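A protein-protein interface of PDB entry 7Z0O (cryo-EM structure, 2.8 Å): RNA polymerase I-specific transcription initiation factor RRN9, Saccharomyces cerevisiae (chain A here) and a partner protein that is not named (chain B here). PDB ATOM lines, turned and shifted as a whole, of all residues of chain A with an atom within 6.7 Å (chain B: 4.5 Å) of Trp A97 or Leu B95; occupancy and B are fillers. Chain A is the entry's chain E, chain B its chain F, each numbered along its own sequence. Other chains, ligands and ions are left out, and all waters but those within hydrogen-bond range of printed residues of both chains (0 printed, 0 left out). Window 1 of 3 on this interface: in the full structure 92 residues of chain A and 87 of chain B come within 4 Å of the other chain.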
ATOM      1  N   LEU A  56      18.926 -24.326  31.119  1.00  0.00           N
ATOM      2  CA  LEU A  56      17.653 -24.393  30.419  1.00  0.00           C
ATOM      3  C   LEU A  56      17.732 -23.859  28.998  1.00  0.00           C
ATOM      4  O   LEU A  56      16.951 -24.289  28.145  1.00  0.00           O
ATOM      5  CB  LEU A  56      16.591 -23.616  31.198  1.00  0.00           C
ATOM      6  CG  LEU A  56      15.149 -23.701  30.697  1.00  0.00           C
ATOM      7  CD1 LEU A  56      14.575 -25.082  30.950  1.00  0.00           C
ATOM      8  CD2 LEU A  56      14.294 -22.632  31.351  1.00  0.00           C
ATOM      9  N   SER A  57      18.665 -22.945  28.725  1.00  0.00           N
ATOM     10  CA  SER A  57      18.726 -22.314  27.409  1.00  0.00           C
ATOM     11  C   SER A  57      18.981 -23.337  26.309  1.00  0.00           C
ATOM     12  O   SER A  57      18.359 -23.281  25.242  1.00  0.00           O
ATOM     13  CB  SER A  57      19.809 -21.238  27.396  1.00  0.00           C
ATOM     14  OG  SER A  57      19.514 -20.210  28.323  1.00  0.00           O
ATOM     15  N   LEU A  60      15.789 -25.465  25.848  1.00  0.00           N
ATOM     16  CA  LEU A  60      14.792 -24.735  25.075  1.00  0.00           C
ATOM     17  C   LEU A  60      15.185 -24.672  23.608  1.00  0.00           C
ATOM     18  O   LEU A  60      14.330 -24.775  22.723  1.00  0.00           O
ATOM     19  CB  LEU A  60      14.609 -23.327  25.635  1.00  0.00           C
ATOM     20  CG  LEU A  60      14.124 -23.201  27.076  1.00  0.00           C
ATOM     21  CD1 LEU A  60      14.176 -21.752  27.518  1.00  0.00           C
ATOM     22  CD2 LEU A  60      12.721 -23.757  27.216  1.00  0.00           C
ATOM     23  N   ASP A  92       2.440 -28.233  22.499  1.00  0.00           N
ATOM     24  CA  ASP A  92       2.771 -26.838  22.764  1.00  0.00           C
ATOM     25  C   ASP A  92       3.094 -26.615  24.233  1.00  0.00           C
ATOM     26  O   ASP A  92       3.946 -25.784  24.562  1.00  0.00           O
ATOM     27  CB  ASP A  92       1.618 -25.930  22.337  1.00  0.00           C
ATOM     28  CG  ASP A  92       1.045 -26.311  20.989  1.00  0.00           C
ATOM     29  OD1 ASP A  92       0.756 -27.508  20.779  1.00  0.00           O
ATOM     30  OD2 ASP A  92       0.881 -25.412  20.138  1.00  0.00           O
ATOM     31  N   ASN A  93       2.435 -27.353  25.128  1.00  0.00           N
ATOM     32  CA  ASN A  93       2.669 -27.188  26.555  1.00  0.00           C
ATOM     33  C   ASN A  93       4.020 -27.726  27.002  1.00  0.00           C
ATOM     34  O   ASN A  93       4.306 -27.697  28.202  1.00  0.00           O
ATOM     35  CB  ASN A  93       1.555 -27.864  27.356  1.00  0.00           C
ATOM     36  CG  ASN A  93       1.320 -29.300  26.938  1.00  0.00           C
ATOM     37  OD1 ASN A  93       2.262 -30.060  26.721  1.00  0.00           O
ATOM     38  ND2 ASN A  93       0.055 -29.681  26.828  1.00  0.00           N
ATOM     39  N   THR A  95       6.895 -26.316  26.126  1.00  0.00           N
ATOM     40  CA  THR A  95       7.661 -25.110  26.402  1.00  0.00           C
ATOM     41  C   THR A  95       6.795 -23.890  26.679  1.00  0.00           C
ATOM     42  O   THR A  95       7.342 -22.816  26.951  1.00  0.00           O
ATOM     43  CB  THR A  95       8.603 -24.793  25.234  1.00  0.00           C
ATOM     44  OG1 THR A  95       7.836 -24.577  24.045  1.00  0.00           O
ATOM     45  CG2 THR A  95       9.573 -25.934  25.002  1.00  0.00           C
ATOM     46  N   SER A  96       5.474 -24.014  26.618  1.00  0.00           N
ATOM     47  CA  SER A  96       4.606 -22.868  26.846  1.00  0.00           C
ATOM     48  C   SER A  96       4.699 -22.398  28.292  1.00  0.00           C
ATOM     49  O   SER A  96       4.804 -23.205  29.220  1.00  0.00           O
ATOM     50  CB  SER A  96       3.162 -23.220  26.499  1.00  0.00           C
ATOM     51  OG  SER A  96       2.568 -23.987  27.529  1.00  0.00           O
ATOM     52  N   TRP A  97       4.658 -21.084  28.480  1.00  0.00           N
ATOM     53  CA  TRP A  97       4.816 -20.479  29.795  1.00  0.00           C
ATOM     54  C   TRP A  97       4.213 -19.083  29.754  1.00  0.00           C
ATOM     55  O   TRP A  97       4.096 -18.488  28.677  1.00  0.00           O
ATOM     56  CB  TRP A  97       6.297 -20.413  30.196  1.00  0.00           C
ATOM     57  CG  TRP A  97       7.120 -19.575  29.273  1.00  0.00           C
ATOM     58  CD1 TRP A  97       7.659 -19.958  28.084  1.00  0.00           C
ATOM     59  CD2 TRP A  97       7.492 -18.206  29.459  1.00  0.00           C
ATOM     60  NE1 TRP A  97       8.348 -18.918  27.518  1.00  0.00           N
ATOM     61  CE2 TRP A  97       8.261 -17.829  28.343  1.00  0.00           C
ATOM     62  CE3 TRP A  97       7.253 -17.264  30.462  1.00  0.00           C
ATOM     63  CZ2 TRP A  97       8.789 -16.550  28.199  1.00  0.00           C
ATOM     64  CZ3 TRP A  97       7.776 -15.998  30.317  1.00  0.00           C
ATOM     65  CH2 TRP A  97       8.536 -15.651  29.196  1.00  0.00           C
ATOM     66  N   PRO A  98       3.814 -18.530  30.911  1.00  0.00           N
ATOM     67  CA  PRO A  98       3.741 -19.140  32.241  1.00  0.00           C
ATOM     68  C   PRO A  98       2.440 -19.901  32.469  1.00  0.00           C
ATOM     69  O   PRO A  98       1.478 -19.694  31.735  1.00  0.00           O
ATOM     70  CB  PRO A  98       3.831 -17.938  33.173  1.00  0.00           C
ATOM     71  CG  PRO A  98       3.176 -16.856  32.415  1.00  0.00           C
ATOM     72  CD  PRO A  98       3.502 -17.092  30.964  1.00  0.00           C
ATOM     73  N   ASN A  99       2.413 -20.761  33.480  1.00  0.00           N
ATOM     74  CA  ASN A  99       1.243 -21.562  33.801  1.00  0.00           C
ATOM     75  C   ASN A  99       0.918 -21.438  35.280  1.00  0.00           C
ATOM     76  O   ASN A  99       1.799 -21.130  36.089  1.00  0.00           O
ATOM     77  CB  ASN A  99       1.466 -23.044  33.464  1.00  0.00           C
ATOM     78  CG  ASN A  99       2.062 -23.246  32.092  1.00  0.00           C
ATOM     79  OD1 ASN A  99       1.702 -22.556  31.145  1.00  0.00           O
ATOM     80  ND2 ASN A  99       2.973 -24.203  31.976  1.00  0.00           N
ATOM     81  N   THR A 102       3.631 -25.644  37.212  1.00  0.00           N
ATOM     82  CA  THR A 102       5.077 -25.434  37.066  1.00  0.00           C
ATOM     83  C   THR A 102       5.543 -24.138  37.731  1.00  0.00           C
ATOM     84  O   THR A 102       6.206 -23.291  37.130  1.00  0.00           O
ATOM     85  CB  THR A 102       5.517 -25.503  35.592  1.00  0.00           C
ATOM     86  OG1 THR A 102       6.927 -25.260  35.501  1.00  0.00           O
ATOM     87  CG2 THR A 102       4.786 -24.504  34.701  1.00  0.00           C
ATOM     88  N   PHE A 187       6.024  -6.719  30.152  1.00  0.00           N
ATOM     89  CA  PHE A 187       4.928  -7.677  30.223  1.00  0.00           C
ATOM     90  C   PHE A 187       3.582  -6.974  30.308  1.00  0.00           C
ATOM     91  O   PHE A 187       2.593  -7.445  29.738  1.00  0.00           O
ATOM     92  CB  PHE A 187       5.129  -8.609  31.414  1.00  0.00           C
ATOM     93  CG  PHE A 187       6.140  -9.685  31.170  1.00  0.00           C
ATOM     94  CD1 PHE A 187       5.866 -10.724  30.301  1.00  0.00           C
ATOM     95  CD2 PHE A 187       7.369  -9.654  31.800  1.00  0.00           C
ATOM     96  CE1 PHE A 187       6.796 -11.714  30.072  1.00  0.00           C
ATOM     97  CE2 PHE A 187       8.303 -10.642  31.575  1.00  0.00           C
ATOM     98  CZ  PHE A 187       8.016 -11.672  30.709  1.00  0.00           C
ATOM     99  N   LYS A 228      -0.297 -16.464  21.152  1.00  0.00           N
ATOM    100  CA  LYS A 228       1.031 -17.062  21.165  1.00  0.00           C
ATOM    101  C   LYS A 228       2.085 -16.059  20.717  1.00  0.00           C
ATOM    102  O   LYS A 228       1.898 -15.345  19.734  1.00  0.00           O
ATOM    103  CB  LYS A 228       1.072 -18.301  20.272  1.00  0.00           C
ATOM    104  CG  LYS A 228       0.237 -19.457  20.784  1.00  0.00           C
ATOM    105  CD  LYS A 228       0.797 -20.008  22.083  1.00  0.00           C
ATOM    106  CE  LYS A 228       2.237 -20.461  21.917  1.00  0.00           C
ATOM    107  NZ  LYS A 228       2.653 -21.369  23.018  1.00  0.00           N
ATOM    108  N   LEU A 234       8.810 -10.692  20.604  1.00  0.00           N
ATOM    109  CA  LEU A 234       9.670 -10.075  21.609  1.00  0.00           C
ATOM    110  C   LEU A 234      10.555  -9.001  20.991  1.00  0.00           C
ATOM    111  O   LEU A 234      10.786  -7.952  21.603  1.00  0.00           O
ATOM    112  CB  LEU A 234      10.519 -11.141  22.299  1.00  0.00           C
ATOM    113  CG  LEU A 234      10.024 -11.630  23.660  1.00  0.00           C
ATOM    114  CD1 LEU A 234      10.089 -10.514  24.684  1.00  0.00           C
ATOM    115  CD2 LEU A 234       8.613 -12.179  23.556  1.00  0.00           C
ATOM    116  N   TYR A 256      18.376 -18.884  15.023  1.00  0.00           N
ATOM    117  CA  TYR A 256      17.131 -19.486  14.571  1.00  0.00           C
ATOM    118  C   TYR A 256      17.086 -19.761  13.074  1.00  0.00           C
ATOM    119  O   TYR A 256      16.232 -20.535  12.634  1.00  0.00           O
ATOM    120  CB  TYR A 256      15.950 -18.596  14.960  1.00  0.00           C
ATOM    121  CG  TYR A 256      15.808 -18.405  16.450  1.00  0.00           C
ATOM    122  CD1 TYR A 256      15.777 -19.492  17.309  1.00  0.00           C
ATOM    123  CD2 TYR A 256      15.707 -17.136  17.000  1.00  0.00           C
ATOM    124  CE1 TYR A 256      15.649 -19.322  18.667  1.00  0.00           C
ATOM    125  CE2 TYR A 256      15.578 -16.956  18.357  1.00  0.00           C
ATOM    126  CZ  TYR A 256      15.549 -18.051  19.186  1.00  0.00           C
ATOM    127  OH  TYR A 256      15.420 -17.870  20.541  1.00  0.00           O
ATOM    128  N   TYR B   6      10.578 -27.450  31.988  1.00  0.00           N
ATOM    129  CA  TYR B   6      10.979 -26.786  33.223  1.00  0.00           C
ATOM    130  C   TYR B   6      11.107 -27.783  34.365  1.00  0.00           C
ATOM    131  O   TYR B   6      12.058 -27.713  35.152  1.00  0.00           O
ATOM    132  CB  TYR B   6       9.978 -25.687  33.567  1.00  0.00           C
ATOM    133  CG  TYR B   6       9.631 -24.828  32.380  1.00  0.00           C
ATOM    134  CD1 TYR B   6      10.616 -24.130  31.700  1.00  0.00           C
ATOM    135  CD2 TYR B   6       8.328 -24.731  31.925  1.00  0.00           C
ATOM    136  CE1 TYR B   6      10.311 -23.351  30.609  1.00  0.00           C
ATOM    137  CE2 TYR B   6       8.013 -23.955  30.834  1.00  0.00           C
ATOM    138  CZ  TYR B   6       9.009 -23.268  30.180  1.00  0.00           C
ATOM    139  OH  TYR B   6       8.705 -22.492  29.092  1.00  0.00           O
ATOM    140  N   LEU B  68      17.862 -18.614  32.882  1.00  0.00           N
ATOM    141  CA  LEU B  68      16.493 -18.491  32.399  1.00  0.00           C
ATOM    142  C   LEU B  68      15.477 -19.051  33.383  1.00  0.00           C
ATOM    143  O   LEU B  68      14.296 -18.705  33.297  1.00  0.00           O
ATOM    144  CB  LEU B  68      16.355 -19.186  31.046  1.00  0.00           C
ATOM    145  CG  LEU B  68      16.947 -18.434  29.853  1.00  0.00           C
ATOM    146  CD1 LEU B  68      16.474 -19.047  28.550  1.00  0.00           C
ATOM    147  CD2 LEU B  68      16.587 -16.961  29.913  1.00  0.00           C
ATOM    148  N   HIS B  72      12.157 -17.205  34.268  1.00  0.00           N
ATOM    149  CA  HIS B  72      10.881 -17.902  34.156  1.00  0.00           C
ATOM    150  C   HIS B  72      10.072 -17.796  35.441  1.00  0.00           C
ATOM    151  O   HIS B  72       8.856 -17.579  35.401  1.00  0.00           O
ATOM    152  CB  HIS B  72      11.114 -19.366  33.789  1.00  0.00           C
ATOM    153  CG  HIS B  72       9.864 -20.187  33.776  1.00  0.00           C
ATOM    154  ND1 HIS B  72       9.407 -20.863  34.886  1.00  0.00           N
ATOM    155  CD2 HIS B  72       8.969 -20.432  32.792  1.00  0.00           C
ATOM    156  CE1 HIS B  72       8.287 -21.494  34.583  1.00  0.00           C
ATOM    157  NE2 HIS B  72       8.000 -21.249  33.318  1.00  0.00           N
ATOM    158  N   ALA B  75       8.736 -14.221  35.743  1.00  0.00           N
ATOM    159  CA  ALA B  75       7.647 -14.022  34.796  1.00  0.00           C
ATOM    160  C   ALA B  75       6.401 -14.778  35.229  1.00  0.00           C
ATOM    161  O   ALA B  75       5.278 -14.301  35.038  1.00  0.00           O
ATOM    162  CB  ALA B  75       8.083 -14.456  33.399  1.00  0.00           C
ATOM    163  N   LEU B  86      -1.742 -13.614  30.076  1.00  0.00           N
ATOM    164  CA  LEU B  86      -0.505 -14.061  29.456  1.00  0.00           C
ATOM    165  C   LEU B  86      -0.189 -15.516  29.767  1.00  0.00           C
ATOM    166  O   LEU B  86       0.936 -15.958  29.519  1.00  0.00           O
ATOM    167  CB  LEU B  86       0.655 -13.167  29.892  1.00  0.00           C
ATOM    168  CG  LEU B  86       0.650 -11.756  29.308  1.00  0.00           C
ATOM    169  CD1 LEU B  86       1.669 -10.883  30.012  1.00  0.00           C
ATOM    170  CD2 LEU B  86       0.917 -11.798  27.815  1.00  0.00           C
ATOM    171  N   ASN B  88       0.389 -19.190  29.219  1.00  0.00           N
ATOM    172  CA  ASN B  88       0.719 -20.040  28.078  1.00  0.00           C
ATOM    173  C   ASN B  88       0.872 -19.252  26.782  1.00  0.00           C
ATOM    174  O   ASN B  88       0.707 -19.808  25.693  1.00  0.00           O
ATOM    175  CB  ASN B  88      -0.327 -21.145  27.894  1.00  0.00           C
ATOM    176  CG  ASN B  88      -0.108 -22.313  28.825  1.00  0.00           C
ATOM    177  OD1 ASN B  88       0.781 -23.134  28.609  1.00  0.00           O
ATOM    178  ND2 ASN B  88      -0.914 -22.392  29.875  1.00  0.00           N
ATOM    179  N   ALA B  89       1.200 -17.967  26.869  1.00  0.00           N
ATOM    180  CA  ALA B  89       1.252 -17.103  25.698  1.00  0.00           C
ATOM    181  C   ALA B  89       2.632 -17.028  25.060  1.00  0.00           C
ATOM    182  O   ALA B  89       2.789 -16.334  24.051  1.00  0.00           O
ATOM    183  CB  ALA B  89       0.786 -15.693  26.068  1.00  0.00           C
ATOM    184  N   PHE B  90       3.627 -17.719  25.607  1.00  0.00           N
ATOM    185  CA  PHE B  90       4.989 -17.653  25.103  1.00  0.00           C
ATOM    186  C   PHE B  90       5.504 -19.055  24.816  1.00  0.00           C
ATOM    187  O   PHE B  90       5.004 -20.045  25.356  1.00  0.00           O
ATOM    188  CB  PHE B  90       5.930 -16.958  26.093  1.00  0.00           C
ATOM    189  CG  PHE B  90       5.459 -15.607  26.542  1.00  0.00           C
ATOM    190  CD1 PHE B  90       5.689 -14.488  25.768  1.00  0.00           C
ATOM    191  CD2 PHE B  90       4.801 -15.457  27.747  1.00  0.00           C
ATOM    192  CE1 PHE B  90       5.263 -13.245  26.182  1.00  0.00           C
ATOM    193  CE2 PHE B  90       4.372 -14.217  28.166  1.00  0.00           C
ATOM    194  CZ  PHE B  90       4.604 -13.110  27.382  1.00  0.00           C
ATOM    195  N   ASP B  91       6.516 -19.128  23.960  1.00  0.00           N
ATOM    196  CA  ASP B  91       7.161 -20.381  23.599  1.00  0.00           C
ATOM    197  C   ASP B  91       8.643 -20.314  23.972  1.00  0.00           C
ATOM    198  O   ASP B  91       9.093 -19.386  24.648  1.00  0.00           O
ATOM    199  CB  ASP B  91       6.957 -20.684  22.114  1.00  0.00           C
ATOM    200  CG  ASP B  91       7.815 -19.820  21.220  1.00  0.00           C
ATOM    201  OD1 ASP B  91       8.019 -18.636  21.551  1.00  0.00           O
ATOM    202  OD2 ASP B  91       8.286 -20.327  20.179  1.00  0.00           O
ATOM    203  N   GLU B  92       9.400 -21.321  23.532  1.00  0.00           N
ATOM    204  CA  GLU B  92      10.803 -21.420  23.925  1.00  0.00           C
ATOM    205  C   GLU B  92      11.621 -20.251  23.391  1.00  0.00           C
ATOM    206  O   GLU B  92      12.516 -19.748  24.080  1.00  0.00           O
ATOM    207  CB  GLU B  92      11.389 -22.754  23.455  1.00  0.00           C
ATOM    208  CG  GLU B  92      11.464 -22.931  21.947  1.00  0.00           C
ATOM    209  CD  GLU B  92      10.215 -23.566  21.370  1.00  0.00           C
ATOM    210  OE1 GLU B  92       9.105 -23.213  21.818  1.00  0.00           O
ATOM    211  OE2 GLU B  92      10.341 -24.417  20.466  1.00  0.00           O
ATOM    212  N   THR B  93      11.336 -19.803  22.166  1.00  0.00           N
ATOM    213  CA  THR B  93      12.118 -18.720  21.581  1.00  0.00           C
ATOM    214  C   THR B  93      11.903 -17.408  22.319  1.00  0.00           C
ATOM    215  O   THR B  93      12.813 -16.574  22.377  1.00  0.00           O
ATOM    216  CB  THR B  93      11.773 -18.555  20.103  1.00  0.00           C
ATOM    217  OG1 THR B  93      10.376 -18.275  19.966  1.00  0.00           O
ATOM    218  CG2 THR B  93      12.108 -19.817  19.340  1.00  0.00           C
ATOM    219  N   SER B  94      10.710 -17.199  22.877  1.00  0.00           N
ATOM    220  CA  SER B  94      10.456 -15.979  23.634  1.00  0.00           C
ATOM    221  C   SER B  94      11.319 -15.917  24.886  1.00  0.00           C
ATOM    222  O   SER B  94      11.838 -14.851  25.237  1.00  0.00           O
ATOM    223  CB  SER B  94       8.976 -15.884  23.998  1.00  0.00           C
ATOM    224  OG  SER B  94       8.184 -15.664  22.846  1.00  0.00           O
ATOM    225  N   LEU B  95      11.481 -17.047  25.576  1.00  0.00           N
ATOM    226  CA  LEU B  95      12.290 -17.060  26.789  1.00  0.00           C
ATOM    227  C   LEU B  95      13.768 -16.860  26.476  1.00  0.00           C
ATOM    228  O   LEU B  95      14.478 -16.178  27.222  1.00  0.00           O
ATOM    229  CB  LEU B  95      12.071 -18.365  27.551  1.00  0.00           C
ATOM    230  CG  LEU B  95      12.489 -18.367  29.021  1.00  0.00           C
ATOM    231  CD1 LEU B  95      11.967 -17.133  29.729  1.00  0.00           C
ATOM    232  CD2 LEU B  95      11.995 -19.622  29.710  1.00  0.00           C
ATOM    233  N   ILE B  96      14.251 -17.455  25.384  1.00  0.00           N
ATOM    234  CA  ILE B  96      15.648 -17.276  24.994  1.00  0.00           C
ATOM    235  C   ILE B  96      15.908 -15.825  24.611  1.00  0.00           C
ATOM    236  O   ILE B  96      16.894 -15.215  25.040  1.00  0.00           O
ATOM    237  CB  ILE B  96      16.011 -18.233  23.847  1.00  0.00           C
ATOM    238  CG1 ILE B  96      16.065 -19.673  24.352  1.00  0.00           C
ATOM    239  CG2 ILE B  96      17.337 -17.841  23.226  1.00  0.00           C
ATOM    240  CD1 ILE B  96      16.318 -20.680  23.262  1.00  0.00           C
ATOM    241  N   THR B  97      15.023 -15.248  23.796  1.00  0.00           N
ATOM    242  CA  THR B  97      15.183 -13.856  23.397  1.00  0.00           C
ATOM    243  C   THR B  97      15.046 -12.914  24.584  1.00  0.00           C
ATOM    244  O   THR B  97      15.750 -11.901  24.653  1.00  0.00           O
ATOM    245  CB  THR B  97      14.169 -13.514  22.305  1.00  0.00           C
ATOM    246  OG1 THR B  97      14.594 -14.099  21.070  1.00  0.00           O
ATOM    247  CG2 THR B  97      14.042 -12.011  22.121  1.00  0.00           C
ATOM    248  N   LEU B  98      14.170 -13.241  25.535  1.00  0.00           N
ATOM    249  CA  LEU B  98      14.021 -12.407  26.723  1.00  0.00           C
ATOM    250  C   LEU B  98      15.329 -12.313  27.495  1.00  0.00           C
ATOM    251  O   LEU B  98      15.677 -11.246  28.011  1.00  0.00           O
ATOM    252  CB  LEU B  98      12.910 -12.958  27.613  1.00  0.00           C
ATOM    253  CG  LEU B  98      12.525 -12.114  28.826  1.00  0.00           C
ATOM    254  CD1 LEU B  98      12.143 -10.713  28.392  1.00  0.00           C
ATOM    255  CD2 LEU B  98      11.392 -12.767  29.592  1.00  0.00           C
ATOM    256  N   GLY B  99      16.067 -13.419  27.583  1.00  0.00           N
ATOM    257  CA  GLY B  99      17.364 -13.378  28.237  1.00  0.00           C
ATOM    258  C   GLY B  99      18.354 -12.483  27.517  1.00  0.00           C
ATOM    259  O   GLY B  99      19.117 -11.751  28.149  1.00  0.00           O
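The backbone NH (N) of Ala B89 lies within hydrogen-bond range of the backbone carbonyl oxygen (O) of Trp A97 (3.5 Å). OD1 of Asn A99 sits close to OD1 of Asn B88 (2.8 Å). OG1 of Thr A95 sits at hydrogen-bond distance from OE1 of Glu B92 (2.9 Å). The backbone NH of Phe B90 is in hydrogen-bond range of the backbone carbonyl oxygen of Trp A97 (3.2 Å). O of Thr B93 sits at hydrogen-bond distance from OH of Tyr A256 (3.4 Å). O of Asp B91 sits at hydrogen-bond distance from NE1 of Trp A97, at 3.0 Å. The backbone carbonyl oxygen (O) of Pro A98 lies within hydrogen-bond range of the backbone NH (N) of Asn B88 (2.8 Å). The side-chain hydroxyl (OG) of Ser A96 lies close to the side-chain amide oxygen (OD1) of Asn B88. The side-chain hydroxyl (OH) of Tyr B6 is in hydrogen-bond range of the backbone carbonyl oxygen (O) of Thr A95 (2.6 Å).
O of Thr B93 sits at hydrogen-bond distance from OG1 of Thr B97. The side-chain carboxylate of Asp B91 sits at hydrogen-bond distance from the side-chain hydroxyl of Ser B94, 3.2 Å away. OD1 of Asp B91 is in hydrogen-bond range of OG1 of Thr B93 (2.9 Å). The backbone carbonyl oxygen (O) of Ser A96 lies within hydrogen-bond range of the side-chain amide nitrogen (ND2) of Asn A99 (3.5 Å).
CD1 of Leu B68 touches OG of Ser A57, 3.3 Å away. Leu A60 touches Leu B95 (CD1 to CD2, 3.8 Å). Phe B90 touches Thr A95 (O to O, 3.96 Å). Phe B90 touches Ser A96. Trp A97 touches Asn B88 (O to CA, 3.8 Å). Leu B95 touches Trp A97 (CD1 to CZ2, 3.6 Å). Leu B86 touches Pro A98. CD2 of Phe B90 touches CD of Pro A98, at 3.8 Å. Phe B90 touches Lys A228 (O to NZ, 3.6 Å). Tyr A256 touches Thr B97.
Of the printed residues of chain B, Ser A96 touches Tyr B6, Asn B88 and Phe B90. Printed residues of chain B within 4 Å of Trp A97: Tyr B6, His B72, Ala B75, Asn B88, Ala B89, Phe B90, Asp B91 and Leu B95. Of the printed residues of chain A, Asp B91 touches Trp A97 (3.0 Å). Leu B95 touches two residues of chain A. The nearest residue of chain A that does not touch Leu B95 is Leu A56 (4.1 Å).
Among the printed residues, 39 pairs touch across the chains. Among the printed residues, no Asp or Glu carboxylate lies within 4 Å of a Lys or Arg side-chain nitrogen of the other chain.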
